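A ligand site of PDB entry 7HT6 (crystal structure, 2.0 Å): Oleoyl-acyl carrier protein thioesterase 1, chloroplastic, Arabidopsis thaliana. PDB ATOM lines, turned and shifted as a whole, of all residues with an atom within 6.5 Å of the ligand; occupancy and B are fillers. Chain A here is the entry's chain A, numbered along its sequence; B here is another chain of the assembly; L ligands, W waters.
OD1 of Asn 25 sits at hydrogen-bond distance from OG1 of Thr 27 (3.0 Å). The side-chain amide nitrogen of Asn 25 sits close to the side-chain amino group of Lys 286. The guanidinium group (NH1) of Arg 185 of chain B lies within hydrogen-bond range of the backbone carbonyl oxygen (O) of Leu 204, 2.9 Å away. O of Leu 217 sits at hydrogen-bond distance from OH of Tyr 80, at 2.6 Å. OE2 of Glu 216 lies within salt-bridge range of NH1 of Arg 284, at 3.5 Å. The backbone NH (N) of Arg 185 of chain B lies within hydrogen-bond range of the side-chain carboxylate (OE1) of Glu 205 (2.9 Å). OG1 of Thr 29 lies within hydrogen-bond range of N of Thr 32 (3.2 Å).
An oxygen (O1) of the ligand sits at hydrogen-bond distance from the backbone NH (N) of Val 30, at 2.9 Å. OD1 of Asn 25 sits close to N3 of the ligand, 3.3 Å away.
Residues that only touch the ligand: Thr 27 (3.9 Å), Ala 28 (3.6 Å), Thr 29 (3.5 Å), Tyr 80 (3.5 Å), Leu 204 (3.9 Å), Val 212 (3.5 Å), Glu 216 (3.7 Å), Leu 217 (3.1 Å) and Arg 185 of chain B (3.7 Å). Hydrophobic or aromatic side chains that line the ligand: Val 30, Tyr 80, Leu 204, Val 212 and Leu 217. 11 residues have an atom within 4 Å of the ligand: Asn 25, Thr 27, Ala 28, Thr 29, Val 30, Tyr 80, Leu 204, Val 212, Glu 216, Leu 217 and Arg 185 of chain B. The nearest printed residue that does not touch the ligand is Trp 283 (4.03 Å).
Water W3 lies within hydrogen-bond range of an oxygen (O1) of the ligand (2.5 Å), the side-chain carboxylate of Glu 31 (3.0 Å) and the backbone NH of Val 30 (3.4 Å).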
ATOM      1  N   GLY A  23      18.666 -24.011  29.847  1.00  0.00           N
ATOM      2  CA  GLY A  23      18.397 -25.406  29.550  1.00  0.00           C
ATOM      3  C   GLY A  23      19.609 -26.305  29.577  1.00  0.00           C
ATOM      4  O   GLY A  23      20.670 -25.920  30.075  1.00  0.00           O
ATOM      5  N   SER A  24      19.443 -27.525  29.033  1.00  0.00           N
ATOM      6  CA  SER A  24      20.465 -28.584  28.964  1.00  0.00           C
ATOM      7  C   SER A  24      21.756 -28.119  28.301  1.00  0.00           C
ATOM      8  O   SER A  24      22.829 -28.637  28.629  1.00  0.00           O
ATOM      9  CB  SER A  24      19.920 -29.785  28.193  1.00  0.00           C
ATOM     10  OG  SER A  24      18.556 -30.068  28.480  1.00  0.00           O
ATOM     11  N   ASN A  25      21.680 -27.142  27.393  1.00  0.00           N
ATOM     12  CA  ASN A  25      22.850 -26.608  26.685  1.00  0.00           C
ATOM     13  C   ASN A  25      23.728 -25.678  27.583  1.00  0.00           C
ATOM     14  O   ASN A  25      24.769 -25.209  27.132  1.00  0.00           O
ATOM     15  CB  ASN A  25      22.372 -25.927  25.360  1.00  0.00           C
ATOM     16  CG  ASN A  25      23.412 -25.246  24.483  1.00  0.00           C
ATOM     17  OD1 ASN A  25      23.176 -24.144  23.932  1.00  0.00           O
ATOM     18  ND2 ASN A  25      24.576 -25.854  24.325  1.00  0.00           N
ATOM     19  N   THR A  27      22.863 -22.743  28.542  1.00  0.00           N
ATOM     20  CA  THR A  27      22.519 -21.390  28.127  1.00  0.00           C
ATOM     21  C   THR A  27      20.955 -21.235  28.070  1.00  0.00           C
ATOM     22  O   THR A  27      20.221 -22.233  28.181  1.00  0.00           O
ATOM     23  CB  THR A  27      23.141 -21.081  26.735  1.00  0.00           C
ATOM     24  OG1 THR A  27      22.487 -21.886  25.758  1.00  0.00           O
ATOM     25  CG2 THR A  27      24.629 -21.315  26.672  1.00  0.00           C
ATOM     26  N   ALA A  28      20.451 -20.006  27.811  1.00  0.00           N
ATOM     27  CA  ALA A  28      19.041 -19.742  27.604  1.00  0.00           C
ATOM     28  C   ALA A  28      18.523 -20.594  26.428  1.00  0.00           C
ATOM     29  O   ALA A  28      19.252 -20.872  25.478  1.00  0.00           O
ATOM     30  CB  ALA A  28      18.827 -18.270  27.281  1.00  0.00           C
ATOM     31  N   THR A  29      17.291 -21.051  26.530  1.00  0.00           N
ATOM     32  CA  THR A  29      16.661 -21.839  25.485  1.00  0.00           C
ATOM     33  C   THR A  29      16.017 -20.883  24.448  1.00  0.00           C
ATOM     34  O   THR A  29      15.901 -19.686  24.693  1.00  0.00           O
ATOM     35  CB  THR A  29      15.638 -22.776  26.128  1.00  0.00           C
ATOM     36  OG1 THR A  29      14.729 -21.999  26.921  1.00  0.00           O
ATOM     37  CG2 THR A  29      16.287 -23.850  27.015  1.00  0.00           C
ATOM     38  N   VAL A  30      15.587 -21.428  23.305  1.00  0.00           N
ATOM     39  CA  VAL A  30      14.832 -20.719  22.262  1.00  0.00           C
ATOM     40  C   VAL A  30      13.541 -20.145  22.907  1.00  0.00           C
ATOM     41  O   VAL A  30      13.242 -18.972  22.752  1.00  0.00           O
ATOM     42  CB  VAL A  30      14.521 -21.710  21.134  1.00  0.00           C
ATOM     43  CG1 VAL A  30      13.478 -21.160  20.169  1.00  0.00           C
ATOM     44  CG2 VAL A  30      15.796 -22.099  20.399  1.00  0.00           C
ATOM     45  N   GLU A  31      12.870 -20.963  23.723  1.00  0.00           N
ATOM     46  CA  GLU A  31      11.683 -20.557  24.467  1.00  0.00           C
ATOM     47  C   GLU A  31      11.964 -19.407  25.432  1.00  0.00           C
ATOM     48  O   GLU A  31      11.122 -18.526  25.537  1.00  0.00           O
ATOM     49  CB  GLU A  31      11.095 -21.747  25.225  1.00  0.00           C
ATOM     50  CG  GLU A  31      10.228 -22.634  24.382  1.00  0.00           C
ATOM     51  CD  GLU A  31       9.955 -23.931  25.097  1.00  0.00           C
ATOM     52  OE1 GLU A  31      10.764 -24.882  24.928  1.00  0.00           O
ATOM     53  OE2 GLU A  31       8.959 -23.999  25.849  1.00  0.00           O
ATOM     54  N   THR A  32      13.129 -19.391  26.114  1.00  0.00           N
ATOM     55  CA  THR A  32      13.474 -18.270  26.989  1.00  0.00           C
ATOM     56  C   THR A  32      13.642 -16.974  26.187  1.00  0.00           C
ATOM     57  O   THR A  32      13.138 -15.919  26.596  1.00  0.00           O
ATOM     58  CB  THR A  32      14.713 -18.569  27.860  1.00  0.00           C
ATOM     59  OG1 THR A  32      14.307 -19.455  28.926  1.00  0.00           O
ATOM     60  CG2 THR A  32      15.326 -17.289  28.479  1.00  0.00           C
ATOM     61  N   TYR A  80      23.817 -17.581  22.333  1.00  0.00           N
ATOM     62  CA  TYR A  80      22.848 -17.705  23.424  1.00  0.00           C
ATOM     63  C   TYR A  80      23.446 -17.229  24.739  1.00  0.00           C
ATOM     64  O   TYR A  80      24.523 -17.689  25.137  1.00  0.00           O
ATOM     65  CB  TYR A  80      22.349 -19.156  23.562  1.00  0.00           C
ATOM     66  CG  TYR A  80      21.402 -19.593  22.477  1.00  0.00           C
ATOM     67  CD1 TYR A  80      21.872 -19.997  21.230  1.00  0.00           C
ATOM     68  CD2 TYR A  80      20.025 -19.638  22.690  1.00  0.00           C
ATOM     69  CE1 TYR A  80      21.005 -20.382  20.216  1.00  0.00           C
ATOM     70  CE2 TYR A  80      19.155 -20.086  21.698  1.00  0.00           C
ATOM     71  CZ  TYR A  80      19.646 -20.427  20.450  1.00  0.00           C
ATOM     72  OH  TYR A  80      18.792 -20.824  19.454  1.00  0.00           O
ATOM     73  N   GLY A 201       8.007 -24.796  21.851  1.00  0.00           N
ATOM     74  CA  GLY A 201       8.432 -25.974  22.594  1.00  0.00           C
ATOM     75  C   GLY A 201       7.988 -27.273  21.944  1.00  0.00           C
ATOM     76  O   GLY A 201       8.819 -28.170  21.729  1.00  0.00           O
ATOM     77  N   LEU A 204       9.887 -28.214  18.812  1.00  0.00           N
ATOM     78  CA  LEU A 204      11.213 -28.739  19.167  1.00  0.00           C
ATOM     79  C   LEU A 204      11.188 -30.133  19.840  1.00  0.00           C
ATOM     80  O   LEU A 204      12.228 -30.778  19.918  1.00  0.00           O
ATOM     81  CB  LEU A 204      12.017 -27.725  20.025  1.00  0.00           C
ATOM     82  CG  LEU A 204      12.289 -26.370  19.338  1.00  0.00           C
ATOM     83  CD1 LEU A 204      13.085 -25.446  20.232  1.00  0.00           C
ATOM     84  CD2 LEU A 204      13.008 -26.534  18.026  1.00  0.00           C
ATOM     85  N   GLU A 205      10.014 -30.611  20.273  1.00  0.00           N
ATOM     86  CA  GLU A 205       9.861 -31.918  20.905  1.00  0.00           C
ATOM     87  C   GLU A 205      10.162 -33.066  19.927  1.00  0.00           C
ATOM     88  O   GLU A 205      10.546 -34.163  20.380  1.00  0.00           O
ATOM     89  CB  GLU A 205       8.435 -32.113  21.457  1.00  0.00           C
ATOM     90  CG  GLU A 205       8.202 -31.741  22.912  1.00  0.00           C
ATOM     91  CD  GLU A 205       9.257 -32.177  23.912  1.00  0.00           C
ATOM     92  OE1 GLU A 205      10.072 -31.309  24.308  1.00  0.00           O
ATOM     93  OE2 GLU A 205       9.260 -33.354  24.328  1.00  0.00           O
ATOM     94  N   VAL A 212      19.839 -32.239  19.254  1.00  0.00           N
ATOM     95  CA  VAL A 212      19.682 -31.400  20.446  1.00  0.00           C
ATOM     96  C   VAL A 212      20.981 -31.340  21.291  1.00  0.00           C
ATOM     97  O   VAL A 212      21.371 -30.254  21.740  1.00  0.00           O
ATOM     98  CB  VAL A 212      18.434 -31.888  21.239  1.00  0.00           C
ATOM     99  CG1 VAL A 212      18.485 -31.522  22.722  1.00  0.00           C
ATOM    100  CG2 VAL A 212      17.165 -31.358  20.595  1.00  0.00           C
ATOM    101  N   ASP A 213      21.649 -32.486  21.467  1.00  0.00           N
ATOM    102  CA  ASP A 213      22.866 -32.653  22.272  1.00  0.00           C
ATOM    103  C   ASP A 213      24.141 -32.081  21.641  1.00  0.00           C
ATOM    104  O   ASP A 213      25.067 -31.735  22.373  1.00  0.00           O
ATOM    105  CB  ASP A 213      23.122 -34.143  22.559  1.00  0.00           C
ATOM    106  CG  ASP A 213      22.123 -34.830  23.467  1.00  0.00           C
ATOM    107  OD1 ASP A 213      21.399 -34.114  24.205  1.00  0.00           O
ATOM    108  OD2 ASP A 213      22.057 -36.078  23.440  1.00  0.00           O
ATOM    109  N   HIS A 215      24.032 -29.809  18.637  1.00  0.00           N
ATOM    110  CA  HIS A 215      23.795 -28.605  17.846  1.00  0.00           C
ATOM    111  C   HIS A 215      23.084 -27.503  18.670  1.00  0.00           C
ATOM    112  O   HIS A 215      22.515 -27.770  19.720  1.00  0.00           O
ATOM    113  CB  HIS A 215      22.936 -28.917  16.593  1.00  0.00           C
ATOM    114  CG  HIS A 215      23.620 -29.700  15.509  1.00  0.00           C
ATOM    115  ND1 HIS A 215      24.066 -30.992  15.726  1.00  0.00           N
ATOM    116  CD2 HIS A 215      23.806 -29.386  14.209  1.00  0.00           C
ATOM    117  CE1 HIS A 215      24.539 -31.407  14.559  1.00  0.00           C
ATOM    118  NE2 HIS A 215      24.426 -30.470  13.627  1.00  0.00           N
ATOM    119  N   GLU A 216      23.101 -26.272  18.136  1.00  0.00           N
ATOM    120  CA  GLU A 216      22.389 -25.101  18.647  1.00  0.00           C
ATOM    121  C   GLU A 216      21.474 -24.625  17.527  1.00  0.00           C
ATOM    122  O   GLU A 216      21.856 -24.653  16.360  1.00  0.00           O
ATOM    123  CB  GLU A 216      23.376 -23.972  19.034  1.00  0.00           C
ATOM    124  CG  GLU A 216      24.254 -24.323  20.210  1.00  0.00           C
ATOM    125  CD  GLU A 216      25.105 -23.213  20.796  1.00  0.00           C
ATOM    126  OE1 GLU A 216      25.962 -23.535  21.658  1.00  0.00           O
ATOM    127  OE2 GLU A 216      24.940 -22.032  20.398  1.00  0.00           O
ATOM    128  N   LEU A 217      20.264 -24.189  17.881  1.00  0.00           N
ATOM    129  CA  LEU A 217      19.320 -23.706  16.889  1.00  0.00           C
ATOM    130  C   LEU A 217      19.810 -22.328  16.425  1.00  0.00           C
ATOM    131  O   LEU A 217      20.105 -21.464  17.252  1.00  0.00           O
ATOM    132  CB  LEU A 217      17.878 -23.684  17.434  1.00  0.00           C
ATOM    133  CG  LEU A 217      16.775 -23.272  16.456  1.00  0.00           C
ATOM    134  CD1 LEU A 217      15.479 -24.007  16.754  1.00  0.00           C
ATOM    135  CD2 LEU A 217      16.524 -21.766  16.498  1.00  0.00           C
ATOM    136  N   GLN A 218      19.966 -22.152  15.114  1.00  0.00           N
ATOM    137  CA  GLN A 218      20.386 -20.854  14.571  1.00  0.00           C
ATOM    138  C   GLN A 218      19.167 -20.069  14.059  1.00  0.00           C
ATOM    139  O   GLN A 218      19.072 -18.892  14.361  1.00  0.00           O
ATOM    140  CB  GLN A 218      21.440 -21.026  13.466  1.00  0.00           C
ATOM    141  CG  GLN A 218      21.853 -19.698  12.817  1.00  0.00           C
ATOM    142  CD  GLN A 218      23.274 -19.741  12.318  1.00  0.00           C
ATOM    143  OE1 GLN A 218      23.556 -20.170  11.192  1.00  0.00           O
ATOM    144  NE2 GLN A 218      24.191 -19.306  13.150  1.00  0.00           N
ATOM    145  N   TRP A 283      19.879 -25.641  12.260  1.00  0.00           N
ATOM    146  CA  TRP A 283      20.743 -25.903  13.411  1.00  0.00           C
ATOM    147  C   TRP A 283      22.202 -25.936  13.000  1.00  0.00           C
ATOM    148  O   TRP A 283      22.513 -26.485  11.944  1.00  0.00           O
ATOM    149  CB  TRP A 283      20.349 -27.252  14.044  1.00  0.00           C
ATOM    150  CG  TRP A 283      18.978 -27.278  14.650  1.00  0.00           C
ATOM    151  CD1 TRP A 283      17.788 -27.251  13.980  1.00  0.00           C
ATOM    152  CD2 TRP A 283      18.648 -27.373  16.043  1.00  0.00           C
ATOM    153  NE1 TRP A 283      16.744 -27.254  14.866  1.00  0.00           N
ATOM    154  CE2 TRP A 283      17.240 -27.374  16.142  1.00  0.00           C
ATOM    155  CE3 TRP A 283      19.404 -27.471  17.219  1.00  0.00           C
ATOM    156  CZ2 TRP A 283      16.586 -27.450  17.374  1.00  0.00           C
ATOM    157  CZ3 TRP A 283      18.748 -27.532  18.434  1.00  0.00           C
ATOM    158  CH2 TRP A 283      17.356 -27.539  18.501  1.00  0.00           C
ATOM    159  N   ARG A 284      23.087 -25.374  13.849  1.00  0.00           N
ATOM    160  CA  ARG A 284      24.537 -25.357  13.630  1.00  0.00           C
ATOM    161  C   ARG A 284      25.266 -26.219  14.678  1.00  0.00           C
ATOM    162  O   ARG A 284      24.894 -26.217  15.837  1.00  0.00           O
ATOM    163  CB  ARG A 284      25.074 -23.893  13.570  1.00  0.00           C
ATOM    164  CG  ARG A 284      25.955 -23.416  14.738  1.00  0.00           C
ATOM    165  CD  ARG A 284      25.878 -21.911  14.995  1.00  0.00           C
ATOM    166  NE  ARG A 284      25.136 -21.610  16.224  1.00  0.00           N
ATOM    167  CZ  ARG A 284      24.474 -20.475  16.432  1.00  0.00           C
ATOM    168  NH1 ARG A 284      23.812 -20.283  17.567  1.00  0.00           N
ATOM    169  NH2 ARG A 284      24.468 -19.517  15.521  1.00  0.00           N
ATOM    170  N   LYS A 286      27.751 -27.435  17.485  1.00  0.00           N
ATOM    171  CA  LYS A 286      28.353 -26.689  18.601  1.00  0.00           C
ATOM    172  C   LYS A 286      29.872 -26.569  18.415  1.00  0.00           C
ATOM    173  O   LYS A 286      30.522 -27.554  18.095  1.00  0.00           O
ATOM    174  CB  LYS A 286      28.045 -27.340  19.961  1.00  0.00           C
ATOM    175  CG  LYS A 286      26.574 -27.389  20.337  1.00  0.00           C
ATOM    176  CD  LYS A 286      26.370 -28.258  21.592  1.00  0.00           C
ATOM    177  CE  LYS A 286      24.908 -28.310  21.988  1.00  0.00           C
ATOM    178  NZ  LYS A 286      24.666 -29.065  23.256  1.00  0.00           N
ATOM    179  N   ARG B 185      11.119 -31.166  26.969  1.00  0.00           N
ATOM    180  CA  ARG B 185      12.539 -30.805  27.043  1.00  0.00           C
ATOM    181  C   ARG B 185      12.789 -29.507  27.802  1.00  0.00           C
ATOM    182  O   ARG B 185      13.876 -29.359  28.353  1.00  0.00           O
ATOM    183  CB  ARG B 185      13.181 -30.767  25.663  1.00  0.00           C
ATOM    184  CG  ARG B 185      13.365 -32.134  25.065  1.00  0.00           C
ATOM    185  CD  ARG B 185      14.187 -32.017  23.821  1.00  0.00           C
ATOM    186  NE  ARG B 185      14.446 -33.330  23.241  1.00  0.00           N
ATOM    187  CZ  ARG B 185      14.373 -33.606  21.952  1.00  0.00           C
ATOM    188  NH1 ARG B 185      14.049 -32.661  21.078  1.00  0.00           N
ATOM    189  NH2 ARG B 185      14.627 -34.829  21.515  1.00  0.00           N
ATOM    190  N   ALA B 186      11.764 -28.610  27.895  1.00  0.00           N
ATOM    191  CA  ALA B 186      11.816 -27.345  28.637  1.00  0.00           C
ATOM    192  C   ALA B 186      11.753 -27.570  30.156  1.00  0.00           C
ATOM    193  O   ALA B 186      12.272 -26.746  30.905  1.00  0.00           O
ATOM    194  CB  ALA B 186      10.699 -26.415  28.204  1.00  0.00           C
HETATM  195  N1  LIG L   1      16.554 -26.388  23.260  1.00  0.00           N
HETATM  196  N2  LIG L   1      18.397 -24.690  21.275  1.00  0.00           N
HETATM  197  C1  LIG L   1      15.202 -27.506  25.249  1.00  0.00           C
HETATM  198  C2  LIG L   1      14.705 -27.938  23.866  1.00  0.00           C
HETATM  199  C3  LIG L   1      15.429 -27.199  22.746  1.00  0.00           C
HETATM  200  C4  LIG L   1      16.674 -25.080  22.961  1.00  0.00           C
HETATM  201  C5  LIG L   1      18.024 -24.570  22.555  1.00  0.00           C
HETATM  202  C6  LIG L   1      20.403 -23.586  21.856  1.00  0.00           C
HETATM  203  C7  LIG L   1      18.387 -28.058  23.481  1.00  0.00           C
HETATM  204  C8  LIG L   1      19.583 -24.191  20.933  1.00  0.00           C
HETATM  205  C9  LIG L   1      17.490 -27.056  24.196  1.00  0.00           C
HETATM  206  C10 LIG L   1      16.720 -27.702  25.354  1.00  0.00           C
HETATM  207  C11 LIG L   1      18.838 -23.908  23.463  1.00  0.00           C
HETATM  208  N3  LIG L   1      20.043 -23.436  23.124  1.00  0.00           N
HETATM  209  O1  LIG L   1      15.699 -24.336  22.957  1.00  0.00           O
HETATM  210  O   HOH W   1      19.624 -24.437  26.601  1.00  0.00           O
HETATM  211  O   HOH W   2      20.799 -27.272  21.541  1.00  0.00           O
HETATM  212  O   HOH W   3      13.353 -23.985  23.802  1.00  0.00           O
